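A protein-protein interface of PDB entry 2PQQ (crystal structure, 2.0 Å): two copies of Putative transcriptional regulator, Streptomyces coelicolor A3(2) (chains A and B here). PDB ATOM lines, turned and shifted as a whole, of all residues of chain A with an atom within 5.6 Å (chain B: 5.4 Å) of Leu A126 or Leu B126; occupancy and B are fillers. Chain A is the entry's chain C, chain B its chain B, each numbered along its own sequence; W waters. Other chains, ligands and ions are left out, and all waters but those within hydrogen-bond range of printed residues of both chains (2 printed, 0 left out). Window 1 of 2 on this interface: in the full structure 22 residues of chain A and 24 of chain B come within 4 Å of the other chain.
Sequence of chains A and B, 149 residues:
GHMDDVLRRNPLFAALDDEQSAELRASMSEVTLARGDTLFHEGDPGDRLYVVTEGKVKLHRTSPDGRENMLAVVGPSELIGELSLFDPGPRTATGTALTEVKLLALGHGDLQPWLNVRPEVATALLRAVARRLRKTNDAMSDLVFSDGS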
ATOM      1  N   PHE A  86     -30.001  18.393 -18.774  1.00  0.00           N
ATOM      2  CA  PHE A  86     -29.114  19.497 -19.216  1.00  0.00           C
ATOM      3  C   PHE A  86     -28.262  19.229 -20.467  1.00  0.00           C
ATOM      4  O   PHE A  86     -27.981  20.148 -21.254  1.00  0.00           O
ATOM      5  CB  PHE A  86     -28.217  19.938 -18.061  1.00  0.00           C
ATOM      6  CG  PHE A  86     -28.981  20.290 -16.816  1.00  0.00           C
ATOM      7  CD1 PHE A  86     -29.982  21.253 -16.868  1.00  0.00           C
ATOM      8  CD2 PHE A  86     -28.712  19.641 -15.615  1.00  0.00           C
ATOM      9  CE1 PHE A  86     -30.721  21.603 -15.722  1.00  0.00           C
ATOM     10  CE2 PHE A  86     -29.440  19.961 -14.452  1.00  0.00           C
ATOM     11  CZ  PHE A  86     -30.443  20.966 -14.514  1.00  0.00           C
ATOM     12  N   LEU A 111     -37.261  22.580 -20.563  1.00  0.00           N
ATOM     13  CA  LEU A 111     -36.360  23.318 -19.661  1.00  0.00           C
ATOM     14  C   LEU A 111     -36.386  24.824 -19.919  1.00  0.00           C
ATOM     15  O   LEU A 111     -36.603  25.645 -19.001  1.00  0.00           O
ATOM     16  CB  LEU A 111     -34.935  22.746 -19.754  1.00  0.00           C
ATOM     17  CG  LEU A 111     -33.872  23.219 -18.775  1.00  0.00           C
ATOM     18  CD1 LEU A 111     -34.261  23.004 -17.292  1.00  0.00           C
ATOM     19  CD2 LEU A 111     -32.568  22.510 -19.121  1.00  0.00           C
ATOM     20  N   LEU A 115     -37.398  27.913 -17.472  1.00  0.00           N
ATOM     21  CA  LEU A 115     -36.342  28.860 -17.041  1.00  0.00           C
ATOM     22  C   LEU A 115     -36.405  30.280 -17.612  1.00  0.00           C
ATOM     23  O   LEU A 115     -35.900  31.205 -16.992  1.00  0.00           O
ATOM     24  CB  LEU A 115     -34.947  28.257 -17.292  1.00  0.00           C
ATOM     25  CG  LEU A 115     -34.675  26.996 -16.470  1.00  0.00           C
ATOM     26  CD1 LEU A 115     -33.237  26.589 -16.687  1.00  0.00           C
ATOM     27  CD2 LEU A 115     -34.986  27.264 -14.950  1.00  0.00           C
ATOM     28  N   VAL A 121     -34.282  30.446 -10.458  1.00  0.00           N
ATOM     29  CA  VAL A 121     -34.251  28.998 -10.571  1.00  0.00           C
ATOM     30  C   VAL A 121     -33.024  28.584 -11.395  1.00  0.00           C
ATOM     31  O   VAL A 121     -32.291  27.685 -10.988  1.00  0.00           O
ATOM     32  CB  VAL A 121     -35.587  28.425 -11.150  1.00  0.00           C
ATOM     33  CG1 VAL A 121     -35.438  26.978 -11.538  1.00  0.00           C
ATOM     34  CG2 VAL A 121     -36.722  28.546 -10.098  1.00  0.00           C
ATOM     35  N   ALA A 122     -32.794  29.221 -12.545  1.00  0.00           N
ATOM     36  CA  ALA A 122     -31.656  28.835 -13.374  1.00  0.00           C
ATOM     37  C   ALA A 122     -30.345  28.942 -12.590  1.00  0.00           C
ATOM     38  O   ALA A 122     -29.495  28.081 -12.702  1.00  0.00           O
ATOM     39  CB  ALA A 122     -31.573  29.691 -14.632  1.00  0.00           C
ATOM     40  N   THR A 123     -30.188  30.028 -11.831  1.00  0.00           N
ATOM     41  CA  THR A 123     -28.984  30.223 -11.014  1.00  0.00           C
ATOM     42  C   THR A 123     -28.848  29.154  -9.902  1.00  0.00           C
ATOM     43  O   THR A 123     -27.756  28.698  -9.602  1.00  0.00           O
ATOM     44  CB  THR A 123     -28.911  31.677 -10.400  1.00  0.00           C
ATOM     45  OG1 THR A 123     -29.982  31.881  -9.479  1.00  0.00           O
ATOM     46  CG2 THR A 123     -29.020  32.762 -11.476  1.00  0.00           C
ATOM     47  N   ALA A 124     -29.966  28.810  -9.268  1.00  0.00           N
ATOM     48  CA  ALA A 124     -30.028  27.698  -8.310  1.00  0.00           C
ATOM     49  C   ALA A 124     -29.579  26.349  -8.930  1.00  0.00           C
ATOM     50  O   ALA A 124     -28.799  25.601  -8.336  1.00  0.00           O
ATOM     51  CB  ALA A 124     -31.452  27.575  -7.773  1.00  0.00           C
ATOM     52  N   LEU A 125     -30.065  26.051 -10.124  1.00  0.00           N
ATOM     53  CA  LEU A 125     -29.667  24.798 -10.817  1.00  0.00           C
ATOM     54  C   LEU A 125     -28.190  24.804 -11.172  1.00  0.00           C
ATOM     55  O   LEU A 125     -27.506  23.822 -10.955  1.00  0.00           O
ATOM     56  CB  LEU A 125     -30.495  24.586 -12.071  1.00  0.00           C
ATOM     57  CG  LEU A 125     -31.992  24.536 -11.817  1.00  0.00           C
ATOM     58  CD1 LEU A 125     -32.725  24.495 -13.155  1.00  0.00           C
ATOM     59  CD2 LEU A 125     -32.321  23.362 -10.937  1.00  0.00           C
ATOM     60  N   LEU A 126     -27.692  25.939 -11.665  1.00  0.00           N
ATOM     61  CA  LEU A 126     -26.268  26.077 -11.984  1.00  0.00           C
ATOM     62  C   LEU A 126     -25.387  25.907 -10.737  1.00  0.00           C
ATOM     63  O   LEU A 126     -24.349  25.282 -10.801  1.00  0.00           O
ATOM     64  CB  LEU A 126     -25.999  27.444 -12.669  1.00  0.00           C
ATOM     65  CG  LEU A 126     -26.346  27.505 -14.178  1.00  0.00           C
ATOM     66  CD1 LEU A 126     -26.516  29.003 -14.549  1.00  0.00           C
ATOM     67  CD2 LEU A 126     -25.268  26.802 -15.046  1.00  0.00           C
ATOM     68  N   ARG A 127     -25.814  26.487  -9.612  1.00  0.00           N
ATOM     69  CA  ARG A 127     -25.117  26.339  -8.334  1.00  0.00           C
ATOM     70  C   ARG A 127     -25.048  24.865  -7.971  1.00  0.00           C
ATOM     71  O   ARG A 127     -23.987  24.357  -7.637  1.00  0.00           O
ATOM     72  CB  ARG A 127     -25.828  27.123  -7.223  1.00  0.00           C
ATOM     73  CG  ARG A 127     -25.127  27.013  -5.829  1.00  0.00           C
ATOM     74  CD  ARG A 127     -25.802  27.935  -4.771  1.00  0.00           C
ATOM     75  NE  ARG A 127     -24.837  28.942  -4.371  1.00  0.00           N
ATOM     76  CZ  ARG A 127     -25.025  30.250  -4.439  1.00  0.00           C
ATOM     77  NH1 ARG A 127     -26.183  30.737  -4.861  1.00  0.00           N
ATOM     78  NH2 ARG A 127     -24.060  31.063  -4.048  1.00  0.00           N
ATOM     79  N   ALA A 128     -26.174  24.176  -8.087  1.00  0.00           N
ATOM     80  CA  ALA A 128     -26.281  22.776  -7.689  1.00  0.00           C
ATOM     81  C   ALA A 128     -25.376  21.864  -8.508  1.00  0.00           C
ATOM     82  O   ALA A 128     -24.671  21.012  -7.959  1.00  0.00           O
ATOM     83  CB  ALA A 128     -27.743  22.323  -7.808  1.00  0.00           C
ATOM     84  N   VAL A 129     -25.403  22.015  -9.824  1.00  0.00           N
ATOM     85  CA  VAL A 129     -24.489  21.261 -10.692  1.00  0.00           C
ATOM     86  C   VAL A 129     -23.016  21.592 -10.407  1.00  0.00           C
ATOM     87  O   VAL A 129     -22.172  20.679 -10.249  1.00  0.00           O
ATOM     88  CB  VAL A 129     -24.794  21.504 -12.166  1.00  0.00           C
ATOM     89  CG1 VAL A 129     -23.817  20.704 -13.047  1.00  0.00           C
ATOM     90  CG2 VAL A 129     -26.222  21.104 -12.469  1.00  0.00           C
ATOM     91  N   ALA A 130     -22.697  22.888 -10.364  1.00  0.00           N
ATOM     92  CA  ALA A 130     -21.328  23.320 -10.078  1.00  0.00           C
ATOM     93  C   ALA A 130     -20.782  22.825  -8.727  1.00  0.00           C
ATOM     94  O   ALA A 130     -19.589  22.496  -8.602  1.00  0.00           O
ATOM     95  CB  ALA A 130     -21.245  24.841 -10.137  1.00  0.00           C
ATOM     96  N   ARG A 131     -21.644  22.810  -7.714  1.00  0.00           N
ATOM     97  CA  ARG A 131     -21.269  22.367  -6.359  1.00  0.00           C
ATOM     98  C   ARG A 131     -20.840  20.892  -6.388  1.00  0.00           C
ATOM     99  O   ARG A 131     -19.889  20.509  -5.704  1.00  0.00           O
ATOM    100  CB  ARG A 131     -22.459  22.560  -5.421  1.00  0.00           C
ATOM    101  CG  ARG A 131     -22.259  22.213  -3.938  1.00  0.00           C
ATOM    102  CD  ARG A 131     -23.356  22.909  -3.098  1.00  0.00           C
ATOM    103  NE  ARG A 131     -24.644  22.994  -3.809  1.00  0.00           N
ATOM    104  CZ  ARG A 131     -25.657  23.803  -3.477  1.00  0.00           C
ATOM    105  NH1 ARG A 131     -25.554  24.599  -2.416  1.00  0.00           N
ATOM    106  NH2 ARG A 131     -26.782  23.804  -4.207  1.00  0.00           N
ATOM    107  N   PHE B  86     -20.575  30.091 -10.537  1.00  0.00           N
ATOM    108  CA  PHE B  86     -21.820  29.408 -10.251  1.00  0.00           C
ATOM    109  C   PHE B  86     -21.969  28.970  -8.826  1.00  0.00           C
ATOM    110  O   PHE B  86     -23.090  28.905  -8.312  1.00  0.00           O
ATOM    111  CB  PHE B  86     -21.952  28.178 -11.205  1.00  0.00           C
ATOM    112  CG  PHE B  86     -21.894  28.572 -12.634  1.00  0.00           C
ATOM    113  CD1 PHE B  86     -22.823  29.490 -13.141  1.00  0.00           C
ATOM    114  CD2 PHE B  86     -20.887  28.085 -13.464  1.00  0.00           C
ATOM    115  CE1 PHE B  86     -22.764  29.916 -14.467  1.00  0.00           C
ATOM    116  CE2 PHE B  86     -20.811  28.498 -14.800  1.00  0.00           C
ATOM    117  CZ  PHE B  86     -21.746  29.410 -15.310  1.00  0.00           C
ATOM    118  N   LEU B 111     -24.742  37.387 -12.702  1.00  0.00           N
ATOM    119  CA  LEU B 111     -25.392  36.270 -13.370  1.00  0.00           C
ATOM    120  C   LEU B 111     -26.897  36.454 -13.506  1.00  0.00           C
ATOM    121  O   LEU B 111     -27.421  36.426 -14.612  1.00  0.00           O
ATOM    122  CB  LEU B 111     -25.042  34.949 -12.651  1.00  0.00           C
ATOM    123  CG  LEU B 111     -25.199  33.595 -13.343  1.00  0.00           C
ATOM    124  CD1 LEU B 111     -24.439  33.539 -14.704  1.00  0.00           C
ATOM    125  CD2 LEU B 111     -24.736  32.465 -12.386  1.00  0.00           C
ATOM    126  N   LEU B 115     -29.075  36.765 -17.073  1.00  0.00           N
ATOM    127  CA  LEU B 115     -30.155  35.831 -17.408  1.00  0.00           C
ATOM    128  C   LEU B 115     -31.531  36.490 -17.542  1.00  0.00           C
ATOM    129  O   LEU B 115     -32.364  36.016 -18.307  1.00  0.00           O
ATOM    130  CB  LEU B 115     -30.210  34.681 -16.405  1.00  0.00           C
ATOM    131  CG  LEU B 115     -28.963  33.823 -16.292  1.00  0.00           C
ATOM    132  CD1 LEU B 115     -29.125  32.819 -15.150  1.00  0.00           C
ATOM    133  CD2 LEU B 115     -28.652  33.115 -17.624  1.00  0.00           C
ATOM    134  N   VAL B 121     -29.805  31.886 -22.394  1.00  0.00           N
ATOM    135  CA  VAL B 121     -28.413  31.592 -22.109  1.00  0.00           C
ATOM    136  C   VAL B 121     -28.340  30.552 -20.966  1.00  0.00           C
ATOM    137  O   VAL B 121     -27.374  29.803 -20.866  1.00  0.00           O
ATOM    138  CB  VAL B 121     -27.620  32.912 -21.804  1.00  0.00           C
ATOM    139  CG1 VAL B 121     -26.348  32.637 -21.019  1.00  0.00           C
ATOM    140  CG2 VAL B 121     -27.298  33.643 -23.088  1.00  0.00           C
ATOM    141  N   ALA B 122     -29.376  30.482 -20.138  1.00  0.00           N
ATOM    142  CA  ALA B 122     -29.349  29.603 -18.968  1.00  0.00           C
ATOM    143  C   ALA B 122     -29.126  28.150 -19.390  1.00  0.00           C
ATOM    144  O   ALA B 122     -28.315  27.460 -18.785  1.00  0.00           O
ATOM    145  CB  ALA B 122     -30.631  29.728 -18.165  1.00  0.00           C
ATOM    146  N   THR B 123     -29.806  27.707 -20.451  1.00  0.00           N
ATOM    147  CA  THR B 123     -29.707  26.305 -20.867  1.00  0.00           C
ATOM    148  C   THR B 123     -28.345  26.002 -21.506  1.00  0.00           C
ATOM    149  O   THR B 123     -27.818  24.895 -21.366  1.00  0.00           O
ATOM    150  CB  THR B 123     -30.865  25.901 -21.774  1.00  0.00           C
ATOM    151  OG1 THR B 123     -30.942  26.814 -22.863  1.00  0.00           O
ATOM    152  CG2 THR B 123     -32.187  25.969 -21.003  1.00  0.00           C
ATOM    153  N   ALA B 124     -27.773  26.981 -22.209  1.00  0.00           N
ATOM    154  CA  ALA B 124     -26.422  26.812 -22.751  1.00  0.00           C
ATOM    155  C   ALA B 124     -25.329  26.712 -21.661  1.00  0.00           C
ATOM    156  O   ALA B 124     -24.409  25.919 -21.772  1.00  0.00           O
ATOM    157  CB  ALA B 124     -26.092  27.932 -23.747  1.00  0.00           C
ATOM    158  N   LEU B 125     -25.440  27.492 -20.594  1.00  0.00           N
ATOM    159  CA  LEU B 125     -24.498  27.346 -19.500  1.00  0.00           C
ATOM    160  C   LEU B 125     -24.706  26.044 -18.770  1.00  0.00           C
ATOM    161  O   LEU B 125     -23.725  25.384 -18.428  1.00  0.00           O
ATOM    162  CB  LEU B 125     -24.605  28.524 -18.548  1.00  0.00           C
ATOM    163  CG  LEU B 125     -24.339  29.920 -19.156  1.00  0.00           C
ATOM    164  CD1 LEU B 125     -24.659  30.926 -18.111  1.00  0.00           C
ATOM    165  CD2 LEU B 125     -22.918  30.057 -19.547  1.00  0.00           C
ATOM    166  N   LEU B 126     -25.970  25.681 -18.510  1.00  0.00           N
ATOM    167  CA  LEU B 126     -26.290  24.389 -17.891  1.00  0.00           C
ATOM    168  C   LEU B 126     -25.717  23.229 -18.677  1.00  0.00           C
ATOM    169  O   LEU B 126     -25.177  22.303 -18.078  1.00  0.00           O
ATOM    170  CB  LEU B 126     -27.800  24.194 -17.625  1.00  0.00           C
ATOM    171  CG  LEU B 126     -28.336  25.016 -16.416  1.00  0.00           C
ATOM    172  CD1 LEU B 126     -29.817  25.141 -16.462  1.00  0.00           C
ATOM    173  CD2 LEU B 126     -27.947  24.365 -15.073  1.00  0.00           C
ATOM    174  N   ARG B 127     -25.810  23.274 -20.007  1.00  0.00           N
ATOM    175  CA  ARG B 127     -25.266  22.171 -20.819  1.00  0.00           C
ATOM    176  C   ARG B 127     -23.759  22.072 -20.588  1.00  0.00           C
ATOM    177  O   ARG B 127     -23.211  20.967 -20.420  1.00  0.00           O
ATOM    178  CB  ARG B 127     -25.541  22.374 -22.314  1.00  0.00           C
ATOM    179  CG  ARG B 127     -24.904  21.294 -23.175  1.00  0.00           C
ATOM    180  CD  ARG B 127     -25.638  21.028 -24.439  1.00  0.00           C
ATOM    181  NE  ARG B 127     -25.382  19.634 -24.874  1.00  0.00           N
ATOM    182  CZ  ARG B 127     -26.133  18.935 -25.723  1.00  0.00           C
ATOM    183  NH1 ARG B 127     -25.803  17.669 -26.020  1.00  0.00           N
ATOM    184  NH2 ARG B 127     -27.221  19.476 -26.263  1.00  0.00           N
ATOM    185  N   ALA B 128     -23.109  23.236 -20.575  1.00  0.00           N
ATOM    186  CA  ALA B 128     -21.662  23.285 -20.504  1.00  0.00           C
ATOM    187  C   ALA B 128     -21.189  22.754 -19.132  1.00  0.00           C
ATOM    188  O   ALA B 128     -20.229  22.001 -19.071  1.00  0.00           O
ATOM    189  CB  ALA B 128     -21.173  24.701 -20.727  1.00  0.00           C
ATOM    190  N   VAL B 129     -21.863  23.129 -18.053  1.00  0.00           N
ATOM    191  CA  VAL B 129     -21.440  22.673 -16.726  1.00  0.00           C
ATOM    192  C   VAL B 129     -21.792  21.187 -16.559  1.00  0.00           C
ATOM    193  O   VAL B 129     -20.976  20.398 -16.076  1.00  0.00           O
ATOM    194  CB  VAL B 129     -22.004  23.550 -15.599  1.00  0.00           C
ATOM    195  CG1 VAL B 129     -21.525  23.040 -14.211  1.00  0.00           C
ATOM    196  CG2 VAL B 129     -21.480  24.980 -15.775  1.00  0.00           C
ATOM    197  N   ALA B 130     -22.980  20.802 -17.025  1.00  0.00           N
ATOM    198  CA  ALA B 130     -23.398  19.405 -17.003  1.00  0.00           C
ATOM    199  C   ALA B 130     -22.508  18.476 -17.825  1.00  0.00           C
ATOM    200  O   ALA B 130     -22.338  17.306 -17.457  1.00  0.00           O
ATOM    201  CB  ALA B 130     -24.833  19.280 -17.429  1.00  0.00           C
ATOM    202  N   ARG B 131     -21.969  18.958 -18.947  1.00  0.00           N
ATOM    203  CA  ARG B 131     -21.010  18.152 -19.708  1.00  0.00           C
ATOM    204  C   ARG B 131     -19.729  17.946 -18.883  1.00  0.00           C
ATOM    205  O   ARG B 131     -19.274  16.838 -18.756  1.00  0.00           O
ATOM    206  CB  ARG B 131     -20.707  18.737 -21.091  1.00  0.00           C
ATOM    207  CG  ARG B 131     -20.089  17.739 -22.074  1.00  0.00           C
ATOM    208  CD  ARG B 131     -21.181  16.857 -22.665  1.00  0.00           C
ATOM    209  NE  ARG B 131     -20.763  15.917 -23.697  1.00  0.00           N
ATOM    210  CZ  ARG B 131     -20.637  16.208 -24.993  1.00  0.00           C
ATOM    211  NH1 ARG B 131     -20.882  17.434 -25.449  1.00  0.00           N
ATOM    212  NH2 ARG B 131     -20.265  15.263 -25.842  1.00  0.00           N
HETATM  213  O   HOH W   1     -29.186  22.694 -20.736  1.00  0.00           O
HETATM  214  O   HOH W   2     -25.365  29.967  -9.783  1.00  0.00           O
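Printed residues of chain B within 4 Å of Leu A126: Phe B86, Leu B125 and Leu B126. Of chain A, only Phe A86, Leu A115, Leu A125 and Leu A126 come within 4 Å of Leu B126. Of the printed residues of chain A, Thr B123 touches Leu A111 (3.9 Å). Printed residues of chain B within 4 Å of Leu A125: Leu B126 (3.9 Å). Ala B124 touches none of the printed residues of chain A. Leu B111 touches none of the printed residues of chain A. The nearest printed residue of chain B that does not touch Arg A127 is Leu B126 (6.2 Å).
Among the printed residues, pairs that only touch across the chains: Arg A127 with Phe B86 (3.3 Å), Phe A86 with Arg B127 (3.4 Å), Val A129 with Val B129 (3.5 Å), Phe A86 with Ala B130 (3.5 Å), Ala A130 with Phe B86 (3.6 Å), Leu A126 with Leu B126 (3.6 Å), Ala A122 with Ala B122 (3.7 Å), Thr A123 with Leu B115 (3.7 Å), Leu A115 with Leu B126 (3.7 Å), Phe A86 with Leu B126 (3.7 Å), Leu A126 with Phe B86 (3.8 Å), Leu A126 with Leu B125 (3.8 Å), Leu A111 with Thr B123 (3.9 Å) and Leu A125 with Leu B126 (3.9 Å).
Water W1 bridges the backbone carbonyl oxygen of Thr B123 (2.7 Å) and the backbone carbonyl oxygen of Phe A86 (2.9 Å). Water W2 bridges O of Thr A123 and O of Phe B86.
Of the 14 printed residues of chain B, 9 touch a printed residue of chain A. Printed residues of chain B that touch a printed residue of chain A: Phe B86, Leu B115, Ala B122, Thr B123, Leu B125, Leu B126, Arg B127, Val B129 and Ala B130. Hydrophobic or aromatic side chains of chain B within 4 Å of the printed part of chain A: Phe B86, Leu B115, Ala B122, Leu B125, Leu B126, Val B129 and Ala B130. Of the 14 printed residues of chain A, 10 touch a printed residue of chain B. Hydrophobic or aromatic side chains of chain A within 4 Å of the printed part of chain B: Phe A86, Leu A111, Leu A115, Ala A122, Leu A125, Leu A126, Val A129 and Ala A130. Among the printed residues, 14 pairs touch across the chains. Among the printed residues, no Asp or Glu carboxylate lies within 4 Å of a Lys or Arg side-chain nitrogen of the other chain.
Phe A86 touches Leu B126, and with the chains exchanged Leu A126 touches Phe B86. Ala B122 touches its own counterpart, Ala A122. Thr A123 touches Leu B115, but with the chains exchanged Leu A115 does not touch Thr B123 (4.5 Å). Leu B126 touches its own counterpart, Leu A126.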
